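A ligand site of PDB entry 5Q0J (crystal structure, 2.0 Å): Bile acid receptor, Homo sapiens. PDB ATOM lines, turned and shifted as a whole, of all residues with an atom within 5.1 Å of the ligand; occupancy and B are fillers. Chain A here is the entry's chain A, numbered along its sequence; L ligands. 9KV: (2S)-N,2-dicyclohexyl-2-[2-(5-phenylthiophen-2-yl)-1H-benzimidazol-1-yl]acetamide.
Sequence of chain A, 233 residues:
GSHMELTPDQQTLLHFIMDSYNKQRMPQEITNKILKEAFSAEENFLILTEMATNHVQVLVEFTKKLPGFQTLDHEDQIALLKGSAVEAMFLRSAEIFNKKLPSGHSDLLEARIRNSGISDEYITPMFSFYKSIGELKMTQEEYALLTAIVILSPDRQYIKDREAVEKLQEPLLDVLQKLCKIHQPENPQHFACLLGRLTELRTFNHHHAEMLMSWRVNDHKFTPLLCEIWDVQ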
ATOM      1  N   ILE A  30      32.951  -4.937 -36.812  1.00  0.00           N
ATOM      2  CA  ILE A  30      31.904  -5.140 -35.816  1.00  0.00           C
ATOM      3  C   ILE A  30      30.514  -4.931 -36.420  1.00  0.00           C
ATOM      4  O   ILE A  30      29.616  -5.773 -36.277  1.00  0.00           O
ATOM      5  CB  ILE A  30      32.153  -4.213 -34.608  1.00  0.00           C
ATOM      6  CG1 ILE A  30      33.519  -4.546 -33.987  1.00  0.00           C
ATOM      7  CG2 ILE A  30      31.059  -4.281 -33.611  1.00  0.00           C
ATOM      8  CD1 ILE A  30      34.402  -3.368 -33.653  1.00  0.00           C
ATOM      9  N   THR A  31      30.299  -3.808 -37.116  1.00  0.00           N
ATOM     10  CA  THR A  31      28.965  -3.557 -37.645  1.00  0.00           C
ATOM     11  C   THR A  31      28.634  -4.508 -38.785  1.00  0.00           C
ATOM     12  O   THR A  31      27.467  -4.802 -39.013  1.00  0.00           O
ATOM     13  CB  THR A  31      28.801  -2.097 -38.075  1.00  0.00           C
ATOM     14  OG1 THR A  31      29.806  -1.777 -39.040  1.00  0.00           O
ATOM     15  CG2 THR A  31      28.997  -1.174 -36.858  1.00  0.00           C
ATOM     16  N   ILE A  34      27.024  -7.680 -37.186  1.00  0.00           N
ATOM     17  CA  ILE A  34      25.697  -7.384 -36.642  1.00  0.00           C
ATOM     18  C   ILE A  34      24.683  -7.162 -37.769  1.00  0.00           C
ATOM     19  O   ILE A  34      23.540  -7.618 -37.692  1.00  0.00           O
ATOM     20  CB  ILE A  34      25.786  -6.161 -35.722  1.00  0.00           C
ATOM     21  CG1 ILE A  34      26.706  -6.427 -34.527  1.00  0.00           C
ATOM     22  CG2 ILE A  34      24.414  -5.728 -35.269  1.00  0.00           C
ATOM     23  CD1 ILE A  34      27.155  -5.147 -33.822  1.00  0.00           C
ATOM     24  N   ASN A  44      24.003 -13.309 -29.491  1.00  0.00           N
ATOM     25  CA  ASN A  44      24.443 -11.923 -29.287  1.00  0.00           C
ATOM     26  C   ASN A  44      25.231 -11.768 -27.989  1.00  0.00           C
ATOM     27  O   ASN A  44      26.218 -11.031 -27.940  1.00  0.00           O
ATOM     28  CB  ASN A  44      23.240 -10.980 -29.299  1.00  0.00           C
ATOM     29  CG  ASN A  44      22.742 -10.686 -30.688  1.00  0.00           C
ATOM     30  OD1 ASN A  44      23.525 -10.607 -31.632  1.00  0.00           O
ATOM     31  ND2 ASN A  44      21.426 -10.495 -30.823  1.00  0.00           N
ATOM     32  N   ILE A  47      28.602 -12.924 -28.695  1.00  0.00           N
ATOM     33  CA  ILE A  47      29.308 -11.930 -29.504  1.00  0.00           C
ATOM     34  C   ILE A  47      29.802 -10.790 -28.616  1.00  0.00           C
ATOM     35  O   ILE A  47      30.958 -10.378 -28.713  1.00  0.00           O
ATOM     36  CB  ILE A  47      28.385 -11.441 -30.648  1.00  0.00           C
ATOM     37  CG1 ILE A  47      28.157 -12.605 -31.637  1.00  0.00           C
ATOM     38  CG2 ILE A  47      28.985 -10.206 -31.392  1.00  0.00           C
ATOM     39  CD1 ILE A  47      27.068 -12.374 -32.693  1.00  0.00           C
ATOM     40  N   LEU A  48      28.977 -10.364 -27.661  1.00  0.00           N
ATOM     41  CA  LEU A  48      29.378  -9.298 -26.738  1.00  0.00           C
ATOM     42  C   LEU A  48      30.572  -9.713 -25.891  1.00  0.00           C
ATOM     43  O   LEU A  48      31.559  -8.966 -25.770  1.00  0.00           O
ATOM     44  CB  LEU A  48      28.187  -8.934 -25.840  1.00  0.00           C
ATOM     45  CG  LEU A  48      28.563  -8.002 -24.685  1.00  0.00           C
ATOM     46  CD1 LEU A  48      29.080  -6.690 -25.292  1.00  0.00           C
ATOM     47  CD2 LEU A  48      27.409  -7.764 -23.730  1.00  0.00           C
ATOM     48  N   MET A  51      33.670  -9.819 -28.098  1.00  0.00           N
ATOM     49  CA  MET A  51      34.102  -8.451 -28.426  1.00  0.00           C
ATOM     50  C   MET A  51      34.738  -7.765 -27.241  1.00  0.00           C
ATOM     51  O   MET A  51      35.760  -7.087 -27.381  1.00  0.00           O
ATOM     52  CB  MET A  51      32.908  -7.617 -28.887  1.00  0.00           C
ATOM     53  CG  MET A  51      32.266  -8.013 -30.220  1.00  0.00           C
ATOM     54  SD  MET A  51      33.476  -7.900 -31.504  1.00  0.00           S
ATOM     55  CE  MET A  51      34.063  -6.246 -31.197  1.00  0.00           C
ATOM     56  N   ALA A  52      34.121  -7.904 -26.053  1.00  0.00           N
ATOM     57  CA  ALA A  52      34.565  -7.180 -24.878  1.00  0.00           C
ATOM     58  C   ALA A  52      35.861  -7.752 -24.349  1.00  0.00           C
ATOM     59  O   ALA A  52      36.681  -7.001 -23.807  1.00  0.00           O
ATOM     60  CB  ALA A  52      33.487  -7.190 -23.798  1.00  0.00           C
ATOM     61  N   HIS A  55      38.415  -6.301 -26.543  1.00  0.00           N
ATOM     62  CA  HIS A  55      38.564  -4.876 -26.245  1.00  0.00           C
ATOM     63  C   HIS A  55      39.441  -4.643 -25.006  1.00  0.00           C
ATOM     64  O   HIS A  55      40.330  -3.787 -25.034  1.00  0.00           O
ATOM     65  CB  HIS A  55      37.199  -4.221 -26.072  1.00  0.00           C
ATOM     66  CG  HIS A  55      37.283  -2.787 -25.733  1.00  0.00           C
ATOM     67  ND1 HIS A  55      37.153  -2.321 -24.444  1.00  0.00           N
ATOM     68  CD2 HIS A  55      37.579  -1.708 -26.489  1.00  0.00           C
ATOM     69  CE1 HIS A  55      37.309  -1.015 -24.426  1.00  0.00           C
ATOM     70  NE2 HIS A  55      37.580  -0.617 -25.656  1.00  0.00           N
ATOM     71  N   MET A  89      34.654   0.827 -22.845  1.00  0.00           N
ATOM     72  CA  MET A  89      33.891  -0.008 -23.770  1.00  0.00           C
ATOM     73  C   MET A  89      32.659   0.715 -24.311  1.00  0.00           C
ATOM     74  O   MET A  89      32.291   0.542 -25.483  1.00  0.00           O
ATOM     75  CB  MET A  89      33.500  -1.307 -23.052  1.00  0.00           C
ATOM     76  CG  MET A  89      33.120  -2.413 -23.967  1.00  0.00           C
ATOM     77  SD  MET A  89      31.506  -3.009 -23.502  1.00  0.00           S
ATOM     78  CE  MET A  89      30.609  -1.482 -23.286  1.00  0.00           C
ATOM     79  N   PHE A  90      31.974   1.495 -23.482  1.00  0.00           N
ATOM     80  CA  PHE A  90      30.806   2.207 -23.972  1.00  0.00           C
ATOM     81  C   PHE A  90      31.204   3.379 -24.846  1.00  0.00           C
ATOM     82  O   PHE A  90      30.481   3.734 -25.777  1.00  0.00           O
ATOM     83  CB  PHE A  90      29.942   2.694 -22.807  1.00  0.00           C
ATOM     84  CG  PHE A  90      29.088   1.609 -22.214  1.00  0.00           C
ATOM     85  CD1 PHE A  90      28.009   1.087 -22.929  1.00  0.00           C
ATOM     86  CD2 PHE A  90      29.365   1.094 -20.947  1.00  0.00           C
ATOM     87  CE1 PHE A  90      27.228   0.079 -22.380  1.00  0.00           C
ATOM     88  CE2 PHE A  90      28.580   0.094 -20.409  1.00  0.00           C
ATOM     89  CZ  PHE A  90      27.522  -0.415 -21.121  1.00  0.00           C
ATOM     90  N   ARG A  92      33.824   3.443 -26.806  1.00  0.00           N
ATOM     91  CA  ARG A  92      34.140   2.816 -28.084  1.00  0.00           C
ATOM     92  C   ARG A  92      32.864   2.366 -28.798  1.00  0.00           C
ATOM     93  O   ARG A  92      32.746   2.561 -30.017  1.00  0.00           O
ATOM     94  CB  ARG A  92      35.107   1.646 -27.867  1.00  0.00           C
ATOM     95  CG  ARG A  92      35.452   0.883 -29.177  1.00  0.00           C
ATOM     96  CD  ARG A  92      36.083   1.821 -30.215  1.00  0.00           C
ATOM     97  NE  ARG A  92      36.611   1.113 -31.384  1.00  0.00           N
ATOM     98  CZ  ARG A  92      37.306   1.705 -32.358  1.00  0.00           C
ATOM     99  NH1 ARG A  92      37.548   3.013 -32.287  1.00  0.00           N
ATOM    100  NH2 ARG A  92      37.759   0.998 -33.378  1.00  0.00           N
ATOM    101  N   SER A  93      31.906   1.779 -28.064  1.00  0.00           N
ATOM    102  CA  SER A  93      30.608   1.442 -28.693  1.00  0.00           C
ATOM    103  C   SER A  93      29.921   2.677 -29.264  1.00  0.00           C
ATOM    104  O   SER A  93      29.310   2.620 -30.340  1.00  0.00           O
ATOM    105  CB  SER A  93      29.681   0.748 -27.691  1.00  0.00           C
ATOM    106  OG  SER A  93      30.153  -0.515 -27.302  1.00  0.00           O
ATOM    107  N   ILE A  96      31.615   3.604 -32.556  1.00  0.00           N
ATOM    108  CA  ILE A  96      31.214   2.702 -33.632  1.00  0.00           C
ATOM    109  C   ILE A  96      29.805   3.019 -34.081  1.00  0.00           C
ATOM    110  O   ILE A  96      29.496   3.097 -35.280  1.00  0.00           O
ATOM    111  CB  ILE A  96      31.345   1.241 -33.171  1.00  0.00           C
ATOM    112  CG1 ILE A  96      32.809   0.888 -32.928  1.00  0.00           C
ATOM    113  CG2 ILE A  96      30.674   0.280 -34.153  1.00  0.00           C
ATOM    114  CD1 ILE A  96      32.977  -0.434 -32.171  1.00  0.00           C
ATOM    115  N   PHE A  97      28.905   3.201 -33.117  1.00  0.00           N
ATOM    116  CA  PHE A  97      27.513   3.452 -33.465  1.00  0.00           C
ATOM    117  C   PHE A  97      27.364   4.677 -34.350  1.00  0.00           C
ATOM    118  O   PHE A  97      26.480   4.718 -35.209  1.00  0.00           O
ATOM    119  CB  PHE A  97      26.696   3.625 -32.186  1.00  0.00           C
ATOM    120  CG  PHE A  97      25.230   3.808 -32.418  1.00  0.00           C
ATOM    121  CD1 PHE A  97      24.395   2.729 -32.637  1.00  0.00           C
ATOM    122  CD2 PHE A  97      24.681   5.094 -32.454  1.00  0.00           C
ATOM    123  CE1 PHE A  97      23.031   2.911 -32.845  1.00  0.00           C
ATOM    124  CE2 PHE A  97      23.342   5.292 -32.667  1.00  0.00           C
ATOM    125  CZ  PHE A  97      22.502   4.199 -32.858  1.00  0.00           C
ATOM    126  N   LEU A 109      21.060  -1.205 -37.808  1.00  0.00           N
ATOM    127  CA  LEU A 109      21.956  -1.459 -36.678  1.00  0.00           C
ATOM    128  C   LEU A 109      21.256  -1.129 -35.360  1.00  0.00           C
ATOM    129  O   LEU A 109      21.342  -1.890 -34.394  1.00  0.00           O
ATOM    130  CB  LEU A 109      23.238  -0.633 -36.841  1.00  0.00           C
ATOM    131  CG  LEU A 109      24.321  -0.788 -35.762  1.00  0.00           C
ATOM    132  CD1 LEU A 109      25.113  -2.096 -35.919  1.00  0.00           C
ATOM    133  CD2 LEU A 109      25.267   0.402 -35.742  1.00  0.00           C
ATOM    134  N   ILE A 113      20.437  -3.816 -32.361  1.00  0.00           N
ATOM    135  CA  ILE A 113      20.803  -3.633 -30.966  1.00  0.00           C
ATOM    136  C   ILE A 113      19.571  -3.620 -30.078  1.00  0.00           C
ATOM    137  O   ILE A 113      19.573  -4.219 -28.994  1.00  0.00           O
ATOM    138  CB  ILE A 113      21.682  -2.378 -30.806  1.00  0.00           C
ATOM    139  CG1 ILE A 113      22.997  -2.575 -31.577  1.00  0.00           C
ATOM    140  CG2 ILE A 113      21.961  -2.120 -29.357  1.00  0.00           C
ATOM    141  CD1 ILE A 113      23.793  -1.321 -31.804  1.00  0.00           C
ATOM    142  N   SER A 116      18.645  -7.173 -29.347  1.00  0.00           N
ATOM    143  CA  SER A 116      19.784  -8.051 -29.112  1.00  0.00           C
ATOM    144  C   SER A 116      19.625  -8.939 -27.889  1.00  0.00           C
ATOM    145  O   SER A 116      20.338  -9.944 -27.785  1.00  0.00           O
ATOM    146  CB  SER A 116      21.060  -7.214 -28.938  1.00  0.00           C
ATOM    147  OG  SER A 116      20.935  -6.343 -27.834  1.00  0.00           O
ATOM    148  N   ILE A 118      19.291  -7.308 -24.693  1.00  0.00           N
ATOM    149  CA  ILE A 118      19.414  -6.361 -23.608  1.00  0.00           C
ATOM    150  C   ILE A 118      18.034  -5.939 -23.104  1.00  0.00           C
ATOM    151  O   ILE A 118      17.063  -5.861 -23.866  1.00  0.00           O
ATOM    152  CB  ILE A 118      20.234  -5.161 -24.108  1.00  0.00           C
ATOM    153  CG1 ILE A 118      20.201  -4.022 -23.113  1.00  0.00           C
ATOM    154  CG2 ILE A 118      19.762  -4.716 -25.457  1.00  0.00           C
ATOM    155  CD1 ILE A 118      21.209  -3.064 -23.443  1.00  0.00           C
ATOM    156  N   MET A 126      20.968   3.969 -23.079  1.00  0.00           N
ATOM    157  CA  MET A 126      22.085   3.668 -23.957  1.00  0.00           C
ATOM    158  C   MET A 126      22.025   4.475 -25.242  1.00  0.00           C
ATOM    159  O   MET A 126      23.014   5.061 -25.672  1.00  0.00           O
ATOM    160  CB  MET A 126      22.120   2.184 -24.268  1.00  0.00           C
ATOM    161  CG  MET A 126      23.356   1.798 -25.014  1.00  0.00           C
ATOM    162  SD  MET A 126      23.377   0.034 -25.264  1.00  0.00           S
ATOM    163  CE  MET A 126      21.947  -0.164 -26.304  1.00  0.00           C
ATOM    164  N   TYR A 130      24.499   7.385 -26.738  1.00  0.00           N
ATOM    165  CA  TYR A 130      25.082   7.300 -28.075  1.00  0.00           C
ATOM    166  C   TYR A 130      24.748   8.534 -28.883  1.00  0.00           C
ATOM    167  O   TYR A 130      25.589   9.073 -29.608  1.00  0.00           O
ATOM    168  CB  TYR A 130      24.584   6.057 -28.826  1.00  0.00           C
ATOM    169  CG  TYR A 130      25.117   4.762 -28.280  1.00  0.00           C
ATOM    170  CD1 TYR A 130      26.113   4.756 -27.297  1.00  0.00           C
ATOM    171  CD2 TYR A 130      24.649   3.541 -28.766  1.00  0.00           C
ATOM    172  CE1 TYR A 130      26.625   3.540 -26.803  1.00  0.00           C
ATOM    173  CE2 TYR A 130      25.156   2.333 -28.283  1.00  0.00           C
ATOM    174  CZ  TYR A 130      26.132   2.334 -27.296  1.00  0.00           C
ATOM    175  OH  TYR A 130      26.636   1.144 -26.798  1.00  0.00           O
ATOM    176  N   HIS A 208      26.591  -1.543 -14.601  1.00  0.00           N
ATOM    177  CA  HIS A 208      26.978  -2.482 -15.661  1.00  0.00           C
ATOM    178  C   HIS A 208      26.697  -3.933 -15.278  1.00  0.00           C
ATOM    179  O   HIS A 208      26.301  -4.733 -16.120  1.00  0.00           O
ATOM    180  CB  HIS A 208      28.457  -2.286 -16.036  1.00  0.00           C
ATOM    181  CG  HIS A 208      29.420  -2.954 -15.118  1.00  0.00           C
ATOM    182  ND1 HIS A 208      29.976  -2.315 -14.023  1.00  0.00           N
ATOM    183  CD2 HIS A 208      29.941  -4.204 -15.119  1.00  0.00           C
ATOM    184  CE1 HIS A 208      30.788  -3.143 -13.394  1.00  0.00           C
ATOM    185  NE2 HIS A 208      30.782  -4.299 -14.043  1.00  0.00           N
ATOM    186  N   MET A 211      23.067  -4.625 -15.831  1.00  0.00           N
ATOM    187  CA  MET A 211      22.842  -4.589 -17.270  1.00  0.00           C
ATOM    188  C   MET A 211      23.189  -5.922 -17.938  1.00  0.00           C
ATOM    189  O   MET A 211      22.503  -6.355 -18.864  1.00  0.00           O
ATOM    190  CB  MET A 211      23.659  -3.468 -17.915  1.00  0.00           C
ATOM    191  CG  MET A 211      23.200  -2.064 -17.578  1.00  0.00           C
ATOM    192  SD  MET A 211      24.276  -0.739 -18.192  1.00  0.00           S
ATOM    193  CE  MET A 211      24.122  -1.010 -19.967  1.00  0.00           C
ATOM    194  N   LEU A 212      24.254  -6.578 -17.478  1.00  0.00           N
ATOM    195  CA  LEU A 212      24.669  -7.840 -18.089  1.00  0.00           C
ATOM    196  C   LEU A 212      23.817  -9.007 -17.616  1.00  0.00           C
ATOM    197  O   LEU A 212      23.458  -9.886 -18.421  1.00  0.00           O
ATOM    198  CB  LEU A 212      26.123  -8.114 -17.754  1.00  0.00           C
ATOM    199  CG  LEU A 212      27.094  -7.165 -18.430  1.00  0.00           C
ATOM    200  CD1 LEU A 212      28.368  -7.117 -17.585  1.00  0.00           C
ATOM    201  CD2 LEU A 212      27.327  -7.673 -19.845  1.00  0.00           C
ATOM    202  N   TRP A 215      20.409  -9.452 -19.162  1.00  0.00           N
ATOM    203  CA  TRP A 215      20.356  -9.867 -20.555  1.00  0.00           C
ATOM    204  C   TRP A 215      19.448 -11.078 -20.680  1.00  0.00           C
ATOM    205  O   TRP A 215      19.492 -11.995 -19.845  1.00  0.00           O
ATOM    206  CB  TRP A 215      21.748 -10.184 -21.076  1.00  0.00           C
ATOM    207  CG  TRP A 215      21.894 -10.129 -22.586  1.00  0.00           C
ATOM    208  CD1 TRP A 215      21.455 -11.059 -23.493  1.00  0.00           C
ATOM    209  CD2 TRP A 215      22.563  -9.117 -23.350  1.00  0.00           C
ATOM    210  NE1 TRP A 215      21.804 -10.673 -24.771  1.00  0.00           N
ATOM    211  CE2 TRP A 215      22.480  -9.488 -24.708  1.00  0.00           C
ATOM    212  CE3 TRP A 215      23.208  -7.925 -23.009  1.00  0.00           C
ATOM    213  CZ2 TRP A 215      23.022  -8.717 -25.729  1.00  0.00           C
ATOM    214  CZ3 TRP A 215      23.763  -7.152 -24.024  1.00  0.00           C
ATOM    215  CH2 TRP A 215      23.668  -7.558 -25.376  1.00  0.00           C
ATOM    216  N   TRP A 230      34.759  -6.943 -14.869  1.00  0.00           N
ATOM    217  CA  TRP A 230      33.337  -6.677 -14.693  1.00  0.00           C
ATOM    218  C   TRP A 230      32.965  -7.211 -13.314  1.00  0.00           C
ATOM    219  O   TRP A 230      33.652  -8.074 -12.756  1.00  0.00           O
ATOM    220  CB  TRP A 230      32.534  -7.381 -15.790  1.00  0.00           C
ATOM    221  CG  TRP A 230      32.606  -6.721 -17.108  1.00  0.00           C
ATOM    222  CD1 TRP A 230      33.212  -5.544 -17.405  1.00  0.00           C
ATOM    223  CD2 TRP A 230      32.083  -7.233 -18.342  1.00  0.00           C
ATOM    224  NE1 TRP A 230      33.048  -5.259 -18.742  1.00  0.00           N
ATOM    225  CE2 TRP A 230      32.366  -6.287 -19.335  1.00  0.00           C
ATOM    226  CE3 TRP A 230      31.380  -8.383 -18.684  1.00  0.00           C
ATOM    227  CZ2 TRP A 230      31.979  -6.459 -20.667  1.00  0.00           C
ATOM    228  CZ3 TRP A 230      30.989  -8.558 -20.007  1.00  0.00           C
ATOM    229  CH2 TRP A 230      31.296  -7.601 -20.974  1.00  0.00           C
HETATM  230  N3  9KV L   1      26.803  -0.988 -28.389  1.00  0.00           N
HETATM  231  C4  9KV L   1      26.787  -2.642 -26.570  1.00  0.00           C
HETATM  232  C5  9KV L   1      29.466  -4.660 -28.870  1.00  0.00           C
HETATM  233  C7  9KV L   1      27.951  -4.436 -28.671  1.00  0.00           C
HETATM  234  C8  9KV L   1      27.681  -2.281 -30.064  1.00  0.00           C
HETATM  235  C10 9KV L   1      27.198  -1.027 -29.731  1.00  0.00           C
HETATM  236  C15 9KV L   1      27.232  -3.613 -22.758  1.00  0.00           C
HETATM  237  C17 9KV L   1      31.714  -3.733 -28.514  1.00  0.00           C
HETATM  238  C20 9KV L   1      26.266  -3.724 -21.751  1.00  0.00           C
HETATM  239  C21 9KV L   1      28.566  -3.806 -22.418  1.00  0.00           C
HETATM  240  C22 9KV L   1      25.599  -4.922 -29.507  1.00  0.00           C
HETATM  241  C24 9KV L   1      32.299  -3.749 -27.093  1.00  0.00           C
HETATM  242  C26 9KV L   1      28.095  -1.586 -32.284  1.00  0.00           C
HETATM  243  C28 9KV L   1      28.931  -4.096 -21.114  1.00  0.00           C
HETATM  244  C1  9KV L   1      27.046  -2.206 -27.944  1.00  0.00           C
HETATM  245  C16 9KV L   1      27.058  -5.392 -29.491  1.00  0.00           C
HETATM  246  C18 9KV L   1      28.127  -2.584 -31.321  1.00  0.00           C
HETATM  247  C19 9KV L   1      27.162  -0.016 -30.693  1.00  0.00           C
HETATM  248  C23 9KV L   1      27.114  -6.819 -28.938  1.00  0.00           C
HETATM  249  C25 9KV L   1      32.250  -2.557 -29.297  1.00  0.00           C
HETATM  250  C27 9KV L   1      27.617  -0.318 -31.980  1.00  0.00           C
HETATM  251  C30 9KV L   1      26.262  -7.779 -29.786  1.00  0.00           C
HETATM  252  C31 9KV L   1      24.661  -5.903 -30.309  1.00  0.00           C
HETATM  253  C32 9KV L   1      33.774  -2.568 -29.327  1.00  0.00           C
HETATM  254  C33 9KV L   1      33.841  -3.662 -27.092  1.00  0.00           C
HETATM  255  C35 9KV L   1      34.345  -2.516 -27.924  1.00  0.00           C
HETATM  256  C36 9KV L   1      24.796  -7.335 -29.837  1.00  0.00           C
HETATM  257  N13 9KV L   1      30.255  -3.691 -28.420  1.00  0.00           N
HETATM  258  N2  9KV L   1      27.569  -3.034 -28.878  1.00  0.00           N
HETATM  259  O14 9KV L   1      29.885  -5.661 -29.414  1.00  0.00           O
HETATM  260  C11 9KV L   1      25.571  -3.063 -26.076  1.00  0.00           C
HETATM  261  C12 9KV L   1      25.605  -3.431 -24.724  1.00  0.00           C
HETATM  262  C29 9KV L   1      26.646  -4.009 -20.449  1.00  0.00           C
HETATM  263  C34 9KV L   1      27.964  -4.197 -20.126  1.00  0.00           C
HETATM  264  C9  9KV L   1      26.840  -3.307 -24.151  1.00  0.00           C
HETATM  265  S6  9KV L   1      28.002  -2.716 -25.331  1.00  0.00           S
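The side-chain hydroxyl (OH) of Tyr 130 sits at hydrogen-bond distance from a nitrogen (N3) of the ligand.
A nitrogen (N13) of the ligand sits at hydrogen-bond distance from the side-chain hydroxyl of Ser 93, 3.4 Å away.
OH of Tyr 130 is in hydrogen-bond range of SD of Met 126 (3.8 Å).
The side-chain hydroxyl of Ser 93 is in hydrogen-bond range of the backbone carbonyl oxygen of Met 89, 3.0 Å away.
O of Ser 116 sits at hydrogen-bond distance from ND2 of Asn 44, 3.3 Å away.
The backbone carbonyl oxygen (O) of Ile 113 sits at hydrogen-bond distance from the side-chain hydroxyl (OG) of Ser 116 (2.8 Å).
The backbone carbonyl oxygen of Ser 116 sits at hydrogen-bond distance from the indole nitrogen of Trp 215.
Ile 34 touches the ligand.
Asn 44 touches the ligand.
Ile 47 touches the ligand.
CB of Leu 48 touches C23 of the ligand (3.9 Å).
CG of Met 51 touches O14 of the ligand (3.4 Å).
His 55 touches the ligand.
CE of Met 89 touches C21 of the ligand (3.2 Å).
CZ of Phe 90 touches C20 of the ligand, at 3.6 Å.
Arg 92 touches the ligand.
Ile 96 touches the ligand.
N of Phe 97 touches C27 of the ligand (3.9 Å).
Ile 113 touches the ligand (CD1 to C19, 3.8 Å).
Ser 116 touches the ligand.
Met 126 touches the ligand.
CE of Met 211 touches C20 of the ligand (3.9 Å).
Leu 212 touches the ligand (CG to C34, 3.5 Å).
Trp 230 touches the ligand.
Hydrophobic or aromatic side chains within 4 Å of the ligand: Ile 34, Ile 47, Leu 48, Met 51, His 55, Met 89, Phe 90, Ile 96, Phe 97, Ile 113, Met 126, Tyr 130, Met 211, Leu 212 and Trp 230.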
